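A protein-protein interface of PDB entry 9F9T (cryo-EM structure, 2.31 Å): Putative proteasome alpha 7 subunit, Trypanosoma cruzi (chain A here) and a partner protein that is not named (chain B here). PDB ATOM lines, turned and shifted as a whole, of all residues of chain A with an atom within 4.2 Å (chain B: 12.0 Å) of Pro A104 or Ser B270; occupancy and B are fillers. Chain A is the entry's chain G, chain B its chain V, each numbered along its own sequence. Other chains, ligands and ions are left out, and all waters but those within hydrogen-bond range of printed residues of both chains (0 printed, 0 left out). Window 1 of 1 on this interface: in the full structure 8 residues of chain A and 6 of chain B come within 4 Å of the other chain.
NH2 of Arg A70 is in salt-bridge range of OE1 of Glu B282 (3.99 Å). NE of Arg A70 is in hydrogen-bond range of OG of Ser B270 (3.2 Å). The guanidinium group (NH2) of Arg A98 sits at hydrogen-bond distance from the backbone carbonyl oxygen (O) of Ser B269 (2.9 Å). The side-chain hydroxyl of Ser B270 is in hydrogen-bond range of the backbone carbonyl oxygen of Cys A220. The backbone carbonyl oxygen (O) of Phe B268 is in hydrogen-bond range of the guanidinium group (NH2) of Arg A70.
Among the printed residues, pairs that only touch across the chains: Arg A70 with Ser B269 (3.7 Å), Gln A71 with Ser B270 (3.6 Å), Arg A98 with Phe B268 (3.4 Å), Thr A103 with Ala B272 (3.7 Å), Pro A104 with Ser B270 (3.7 Å), Pro A104 with Ser B271 (3.7 Å), Pro A104 with Ala B272 (3.8 Å) and Ala A140 with Ser B270 (3.7 Å).
Of the 10 printed residues of chain A, 7 touch a printed residue of chain B. Of the 13 printed residues of chain B, 6 touch a printed residue of chain A. Hydrophobic or aromatic side chains of chain B that line the printed part of chain A: Phe B268 and Ala B272. Among the printed residues, Asp or Glu carboxylates within 4 Å of a Lys or Arg side-chain nitrogen of the other chain: Arg A70 with Glu B282.
Of the printed residues of chain B, Arg A70 touches Phe B268 (3.2 Å), Ser B269 (3.7 Å), Ser B270 (3.2 Å) and Glu B282 (3.99 Å). Gln A71 touches just one residue of chain B: Ser B270. No residue of chain B comes within 4 Å of Ser A97. Of the printed residues of chain B, Thr A103 touches Ala B272 (3.7 Å). Pro A104 touches three residues of chain B. No residue of chain B comes within 4 Å of Ile A105. Cys A220 touches just one residue of chain B: Ser B270 (3.0 Å). Printed residues of chain A within 4 Å of Ser B269: Arg A70 (3.7 Å) and Arg A98 (2.9 Å). Ser B270 touches just these residues of chain A: Arg A70, Gln A71, Pro A104, Ala A140 and Cys A220. Printed residues of chain A within 4 Å of Ser B271: Pro A104 (3.7 Å). Of the printed residues of chain A, Ala B272 touches Thr A103 (3.7 Å) and Pro A104 (3.8 Å). The nearest printed residue of chain A that does not touch Ser B270 is Arg A98 (4.3 Å). The nearest printed residue of chain A that does not touch Glu B282 is Cys A220 (9.8 Å).
OG of Ser B269 sits at hydrogen-bond distance from O of Ser B271. The side-chain hydroxyl (OG) of Ser B271 sits at hydrogen-bond distance from the backbone NH (N) of Lys B273 (2.8 Å). O of Thr A103 sits at hydrogen-bond distance from OG of Ser A97 (2.5 Å). The side-chain amide oxygen of Gln A71 lies within hydrogen-bond range of the guanidinium group of Arg A98, at 2.8 Å.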
ATOM      1  N   ARG A  70      10.884 -24.898 -18.618  1.00  0.00           N
ATOM      2  CA  ARG A  70      11.934 -25.067 -19.611  1.00  0.00           C
ATOM      3  C   ARG A  70      13.256 -25.249 -18.895  1.00  0.00           C
ATOM      4  O   ARG A  70      14.089 -26.007 -19.361  1.00  0.00           O
ATOM      5  CB  ARG A  70      11.950 -23.861 -20.553  1.00  0.00           C
ATOM      6  CG  ARG A  70      13.178 -23.812 -21.428  1.00  0.00           C
ATOM      7  CD  ARG A  70      12.976 -22.812 -22.553  1.00  0.00           C
ATOM      8  NE  ARG A  70      14.326 -22.476 -22.980  1.00  0.00           N
ATOM      9  CZ  ARG A  70      14.816 -22.785 -24.162  1.00  0.00           C
ATOM     10  NH1 ARG A  70      16.117 -22.904 -24.291  1.00  0.00           N
ATOM     11  NH2 ARG A  70      14.006 -23.109 -25.159  1.00  0.00           N
ATOM     12  N   GLN A  71      13.421 -24.562 -17.753  1.00  0.00           N
ATOM     13  CA  GLN A  71      14.695 -24.426 -17.064  1.00  0.00           C
ATOM     14  C   GLN A  71      14.746 -25.122 -15.715  1.00  0.00           C
ATOM     15  O   GLN A  71      15.742 -24.961 -15.001  1.00  0.00           O
ATOM     16  CB  GLN A  71      15.023 -22.954 -16.833  1.00  0.00           C
ATOM     17  CG  GLN A  71      14.317 -22.298 -15.673  1.00  0.00           C
ATOM     18  CD  GLN A  71      12.897 -21.932 -16.000  1.00  0.00           C
ATOM     19  OE1 GLN A  71      12.447 -22.018 -17.133  1.00  0.00           O
ATOM     20  NE2 GLN A  71      12.168 -21.494 -15.007  1.00  0.00           N
ATOM     21  N   SER A  97       4.080 -18.092 -12.894  1.00  0.00           N
ATOM     22  CA  SER A  97       5.084 -17.048 -12.989  1.00  0.00           C
ATOM     23  C   SER A  97       5.224 -16.530 -14.385  1.00  0.00           C
ATOM     24  O   SER A  97       5.334 -15.340 -14.477  1.00  0.00           O
ATOM     25  CB  SER A  97       6.396 -17.427 -12.510  1.00  0.00           C
ATOM     26  OG  SER A  97       7.320 -16.457 -12.906  1.00  0.00           O
ATOM     27  N   ARG A  98       5.165 -17.345 -15.432  1.00  0.00           N
ATOM     28  CA  ARG A  98       5.244 -16.816 -16.807  1.00  0.00           C
ATOM     29  C   ARG A  98       3.967 -16.093 -17.177  1.00  0.00           C
ATOM     30  O   ARG A  98       4.049 -15.012 -17.723  1.00  0.00           O
ATOM     31  CB  ARG A  98       5.520 -17.920 -17.837  1.00  0.00           C
ATOM     32  CG  ARG A  98       6.845 -18.604 -17.537  1.00  0.00           C
ATOM     33  CD  ARG A  98       7.271 -19.696 -18.465  1.00  0.00           C
ATOM     34  NE  ARG A  98       8.665 -20.094 -18.226  1.00  0.00           N
ATOM     35  CZ  ARG A  98       9.683 -19.783 -18.998  1.00  0.00           C
ATOM     36  NH1 ARG A  98       9.508 -18.856 -19.908  1.00  0.00           N
ATOM     37  NH2 ARG A  98      10.892 -20.297 -18.786  1.00  0.00           N
ATOM     38  N   THR A 103       8.025 -13.928 -16.097  1.00  0.00           N
ATOM     39  CA  THR A 103       9.409 -14.230 -15.781  1.00  0.00           C
ATOM     40  C   THR A 103       9.475 -15.739 -15.654  1.00  0.00           C
ATOM     41  O   THR A 103       8.551 -16.316 -15.102  1.00  0.00           O
ATOM     42  CB  THR A 103       9.934 -13.558 -14.466  1.00  0.00           C
ATOM     43  OG1 THR A 103       9.016 -13.400 -13.370  1.00  0.00           O
ATOM     44  CG2 THR A 103      10.460 -12.154 -14.677  1.00  0.00           C
ATOM     45  N   PRO A 104      10.550 -16.418 -16.044  1.00  0.00           N
ATOM     46  CA  PRO A 104      10.741 -17.783 -15.598  1.00  0.00           C
ATOM     47  C   PRO A 104      10.823 -17.738 -14.084  1.00  0.00           C
ATOM     48  O   PRO A 104      11.446 -16.854 -13.539  1.00  0.00           O
ATOM     49  CB  PRO A 104      12.084 -18.217 -16.160  1.00  0.00           C
ATOM     50  CG  PRO A 104      12.464 -17.171 -17.140  1.00  0.00           C
ATOM     51  CD  PRO A 104      11.662 -15.914 -16.824  1.00  0.00           C
ATOM     52  N   ILE A 105      10.199 -18.685 -13.404  1.00  0.00           N
ATOM     53  CA  ILE A 105      10.281 -18.719 -11.956  1.00  0.00           C
ATOM     54  C   ILE A 105      11.721 -18.840 -11.514  1.00  0.00           C
ATOM     55  O   ILE A 105      12.437 -19.714 -11.959  1.00  0.00           O
ATOM     56  CB  ILE A 105       9.418 -19.855 -11.365  1.00  0.00           C
ATOM     57  CG1 ILE A 105       9.118 -19.572  -9.892  1.00  0.00           C
ATOM     58  CG2 ILE A 105       9.991 -21.268 -11.592  1.00  0.00           C
ATOM     59  CD1 ILE A 105       7.817 -20.215  -9.464  1.00  0.00           C
ATOM     60  N   PRO A 106      12.192 -17.984 -10.602  1.00  0.00           N
ATOM     61  CA  PRO A 106      13.431 -18.262  -9.872  1.00  0.00           C
ATOM     62  C   PRO A 106      13.476 -19.570  -9.076  1.00  0.00           C
ATOM     63  O   PRO A 106      12.465 -20.099  -8.645  1.00  0.00           O
ATOM     64  CB  PRO A 106      13.489 -17.125  -8.856  1.00  0.00           C
ATOM     65  CG  PRO A 106      12.690 -15.984  -9.486  1.00  0.00           C
ATOM     66  CD  PRO A 106      11.599 -16.681 -10.283  1.00  0.00           C
ATOM     67  N   ALA A 140      17.681 -20.538 -13.697  1.00  0.00           N
ATOM     68  CA  ALA A 140      16.968 -19.376 -14.207  1.00  0.00           C
ATOM     69  C   ALA A 140      17.864 -18.151 -14.046  1.00  0.00           C
ATOM     70  O   ALA A 140      19.081 -18.310 -13.937  1.00  0.00           O
ATOM     71  CB  ALA A 140      15.658 -19.266 -13.454  1.00  0.00           C
ATOM     72  N   CYS A 220      20.542 -24.168 -21.139  1.00  0.00           N
ATOM     73  CA  CYS A 220      19.787 -24.017 -19.902  1.00  0.00           C
ATOM     74  C   CYS A 220      18.425 -24.685 -19.952  1.00  0.00           C
ATOM     75  O   CYS A 220      17.510 -24.203 -19.315  1.00  0.00           O
ATOM     76  CB  CYS A 220      19.625 -22.547 -19.511  1.00  0.00           C
ATOM     77  SG  CYS A 220      21.033 -21.939 -18.532  1.00  0.00           S
ATOM     78  N   PRO B 266       9.583 -12.528 -28.607  1.00  0.00           N
ATOM     79  CA  PRO B 266      10.797 -13.198 -28.152  1.00  0.00           C
ATOM     80  C   PRO B 266      10.593 -14.701 -28.030  1.00  0.00           C
ATOM     81  O   PRO B 266       9.489 -15.160 -27.749  1.00  0.00           O
ATOM     82  CB  PRO B 266      10.938 -12.581 -26.744  1.00  0.00           C
ATOM     83  CG  PRO B 266       9.496 -12.415 -26.266  1.00  0.00           C
ATOM     84  CD  PRO B 266       8.881 -11.828 -27.515  1.00  0.00           C
ATOM     85  N   PRO B 267      11.659 -15.502 -28.215  1.00  0.00           N
ATOM     86  CA  PRO B 267      11.571 -16.945 -28.080  1.00  0.00           C
ATOM     87  C   PRO B 267      11.368 -17.368 -26.643  1.00  0.00           C
ATOM     88  O   PRO B 267      11.875 -16.734 -25.714  1.00  0.00           O
ATOM     89  CB  PRO B 267      12.968 -17.516 -28.351  1.00  0.00           C
ATOM     90  CG  PRO B 267      13.874 -16.333 -28.614  1.00  0.00           C
ATOM     91  CD  PRO B 267      13.022 -15.070 -28.565  1.00  0.00           C
ATOM     92  N   PHE B 268      10.728 -18.508 -26.504  1.00  0.00           N
ATOM     93  CA  PHE B 268      10.619 -19.213 -25.249  1.00  0.00           C
ATOM     94  C   PHE B 268      12.014 -19.469 -24.682  1.00  0.00           C
ATOM     95  O   PHE B 268      12.820 -20.162 -25.301  1.00  0.00           O
ATOM     96  CB  PHE B 268       9.786 -20.475 -25.513  1.00  0.00           C
ATOM     97  CG  PHE B 268       9.393 -21.245 -24.296  1.00  0.00           C
ATOM     98  CD1 PHE B 268       8.833 -20.601 -23.209  1.00  0.00           C
ATOM     99  CD2 PHE B 268       9.486 -22.631 -24.276  1.00  0.00           C
ATOM    100  CE1 PHE B 268       8.452 -21.313 -22.084  1.00  0.00           C
ATOM    101  CE2 PHE B 268       9.096 -23.344 -23.142  1.00  0.00           C
ATOM    102  CZ  PHE B 268       8.607 -22.675 -22.048  1.00  0.00           C
ATOM    103  N   SER B 269      12.283 -18.909 -23.501  1.00  0.00           N
ATOM    104  CA  SER B 269      13.628 -18.865 -22.954  1.00  0.00           C
ATOM    105  C   SER B 269      13.633 -19.126 -21.466  1.00  0.00           C
ATOM    106  O   SER B 269      12.611 -19.036 -20.793  1.00  0.00           O
ATOM    107  CB  SER B 269      14.290 -17.528 -23.201  1.00  0.00           C
ATOM    108  OG  SER B 269      13.680 -16.565 -22.377  1.00  0.00           O
ATOM    109  N   SER B 270      14.820 -19.426 -20.993  1.00  0.00           N
ATOM    110  CA  SER B 270      15.073 -19.694 -19.594  1.00  0.00           C
ATOM    111  C   SER B 270      15.537 -18.425 -18.840  1.00  0.00           C
ATOM    112  O   SER B 270      16.146 -18.563 -17.767  1.00  0.00           O
ATOM    113  CB  SER B 270      16.144 -20.773 -19.483  1.00  0.00           C
ATOM    114  OG  SER B 270      15.824 -21.931 -20.236  1.00  0.00           O
ATOM    115  N   SER B 271      15.343 -17.219 -19.429  1.00  0.00           N
ATOM    116  CA  SER B 271      15.779 -15.943 -18.854  1.00  0.00           C
ATOM    117  C   SER B 271      14.717 -14.903 -19.131  1.00  0.00           C
ATOM    118  O   SER B 271      14.053 -14.946 -20.150  1.00  0.00           O
ATOM    119  CB  SER B 271      17.096 -15.445 -19.384  1.00  0.00           C
ATOM    120  OG  SER B 271      17.310 -14.026 -19.106  1.00  0.00           O
ATOM    121  N   ALA B 272      14.588 -13.917 -18.250  1.00  0.00           N
ATOM    122  CA  ALA B 272      13.648 -12.831 -18.513  1.00  0.00           C
ATOM    123  C   ALA B 272      14.266 -11.806 -19.459  1.00  0.00           C
ATOM    124  O   ALA B 272      13.539 -10.987 -19.989  1.00  0.00           O
ATOM    125  CB  ALA B 272      13.185 -12.207 -17.212  1.00  0.00           C
ATOM    126  N   LYS B 273      15.558 -11.938 -19.759  1.00  0.00           N
ATOM    127  CA  LYS B 273      16.205 -11.054 -20.704  1.00  0.00           C
ATOM    128  C   LYS B 273      15.589 -11.109 -22.110  1.00  0.00           C
ATOM    129  O   LYS B 273      15.395 -12.164 -22.694  1.00  0.00           O
ATOM    130  CB  LYS B 273      17.704 -11.328 -20.771  1.00  0.00           C
ATOM    131  CG  LYS B 273      18.443 -10.259 -21.533  1.00  0.00           C
ATOM    132  CD  LYS B 273      19.953 -10.431 -21.587  1.00  0.00           C
ATOM    133  CE  LYS B 273      20.667  -9.253 -22.247  1.00  0.00           C
ATOM    134  NZ  LYS B 273      19.848  -8.002 -22.213  1.00  0.00           N
ATOM    135  N   ILE B 274      15.363  -9.921 -22.664  1.00  0.00           N
ATOM    136  CA  ILE B 274      14.773  -9.724 -23.977  1.00  0.00           C
ATOM    137  C   ILE B 274      15.843  -9.209 -24.923  1.00  0.00           C
ATOM    138  O   ILE B 274      16.555  -8.272 -24.579  1.00  0.00           O
ATOM    139  CB  ILE B 274      13.627  -8.705 -23.877  1.00  0.00           C
ATOM    140  CG1 ILE B 274      12.424  -9.284 -23.129  1.00  0.00           C
ATOM    141  CG2 ILE B 274      13.265  -8.150 -25.248  1.00  0.00           C
ATOM    142  CD1 ILE B 274      11.560  -8.238 -22.491  1.00  0.00           C
ATOM    143  N   THR B 275      15.872  -9.782 -26.134  1.00  0.00           N
ATOM    144  CA  THR B 275      16.987  -9.612 -27.047  1.00  0.00           C
ATOM    145  C   THR B 275      16.468  -9.344 -28.466  1.00  0.00           C
ATOM    146  O   THR B 275      16.578  -8.229 -28.980  1.00  0.00           O
ATOM    147  CB  THR B 275      17.927 -10.830 -26.949  1.00  0.00           C
ATOM    148  OG1 THR B 275      17.229 -11.994 -26.488  1.00  0.00           O
ATOM    149  CG2 THR B 275      19.101 -10.570 -26.027  1.00  0.00           C
ATOM    150  N   VAL B 276      15.921 -10.399 -29.086  1.00  0.00           N
ATOM    151  CA  VAL B 276      15.504 -10.382 -30.475  1.00  0.00           C
ATOM    152  C   VAL B 276      14.166 -11.107 -30.629  1.00  0.00           C
ATOM    153  O   VAL B 276      13.752 -11.867 -29.765  1.00  0.00           O
ATOM    154  CB  VAL B 276      16.582 -11.012 -31.370  1.00  0.00           C
ATOM    155  CG1 VAL B 276      17.870 -10.241 -31.243  1.00  0.00           C
ATOM    156  CG2 VAL B 276      16.803 -12.479 -31.058  1.00  0.00           C
ATOM    157  N   GLN B 278      11.987 -13.934 -32.288  1.00  0.00           N
ATOM    158  CA  GLN B 278      12.163 -15.265 -32.861  1.00  0.00           C
ATOM    159  C   GLN B 278      11.872 -15.229 -34.374  1.00  0.00           C
ATOM    160  O   GLN B 278      10.819 -14.722 -34.776  1.00  0.00           O
ATOM    161  CB  GLN B 278      11.216 -16.233 -32.187  1.00  0.00           C
ATOM    162  CG  GLN B 278      11.526 -17.664 -32.500  1.00  0.00           C
ATOM    163  CD  GLN B 278      10.494 -18.663 -32.028  1.00  0.00           C
ATOM    164  OE1 GLN B 278       9.715 -18.455 -31.102  1.00  0.00           O
ATOM    165  NE2 GLN B 278      10.568 -19.838 -32.613  1.00  0.00           N
ATOM    166  N   GLU B 282      11.738 -23.531 -33.590  1.00  0.00           N
ATOM    167  CA  GLU B 282      12.599 -24.399 -32.810  1.00  0.00           C
ATOM    168  C   GLU B 282      12.370 -25.864 -33.212  1.00  0.00           C
ATOM    169  O   GLU B 282      13.382 -26.619 -33.268  1.00  0.00           O
ATOM    170  CB  GLU B 282      12.287 -24.157 -31.338  1.00  0.00           C
ATOM    171  CG  GLU B 282      13.166 -23.091 -30.698  1.00  0.00           C
ATOM    172  CD  GLU B 282      14.544 -23.567 -30.237  1.00  0.00           C
ATOM    173  OE1 GLU B 282      14.699 -23.863 -29.020  1.00  0.00           O
ATOM    174  OE2 GLU B 282      15.479 -23.612 -31.079  1.00  0.00           O
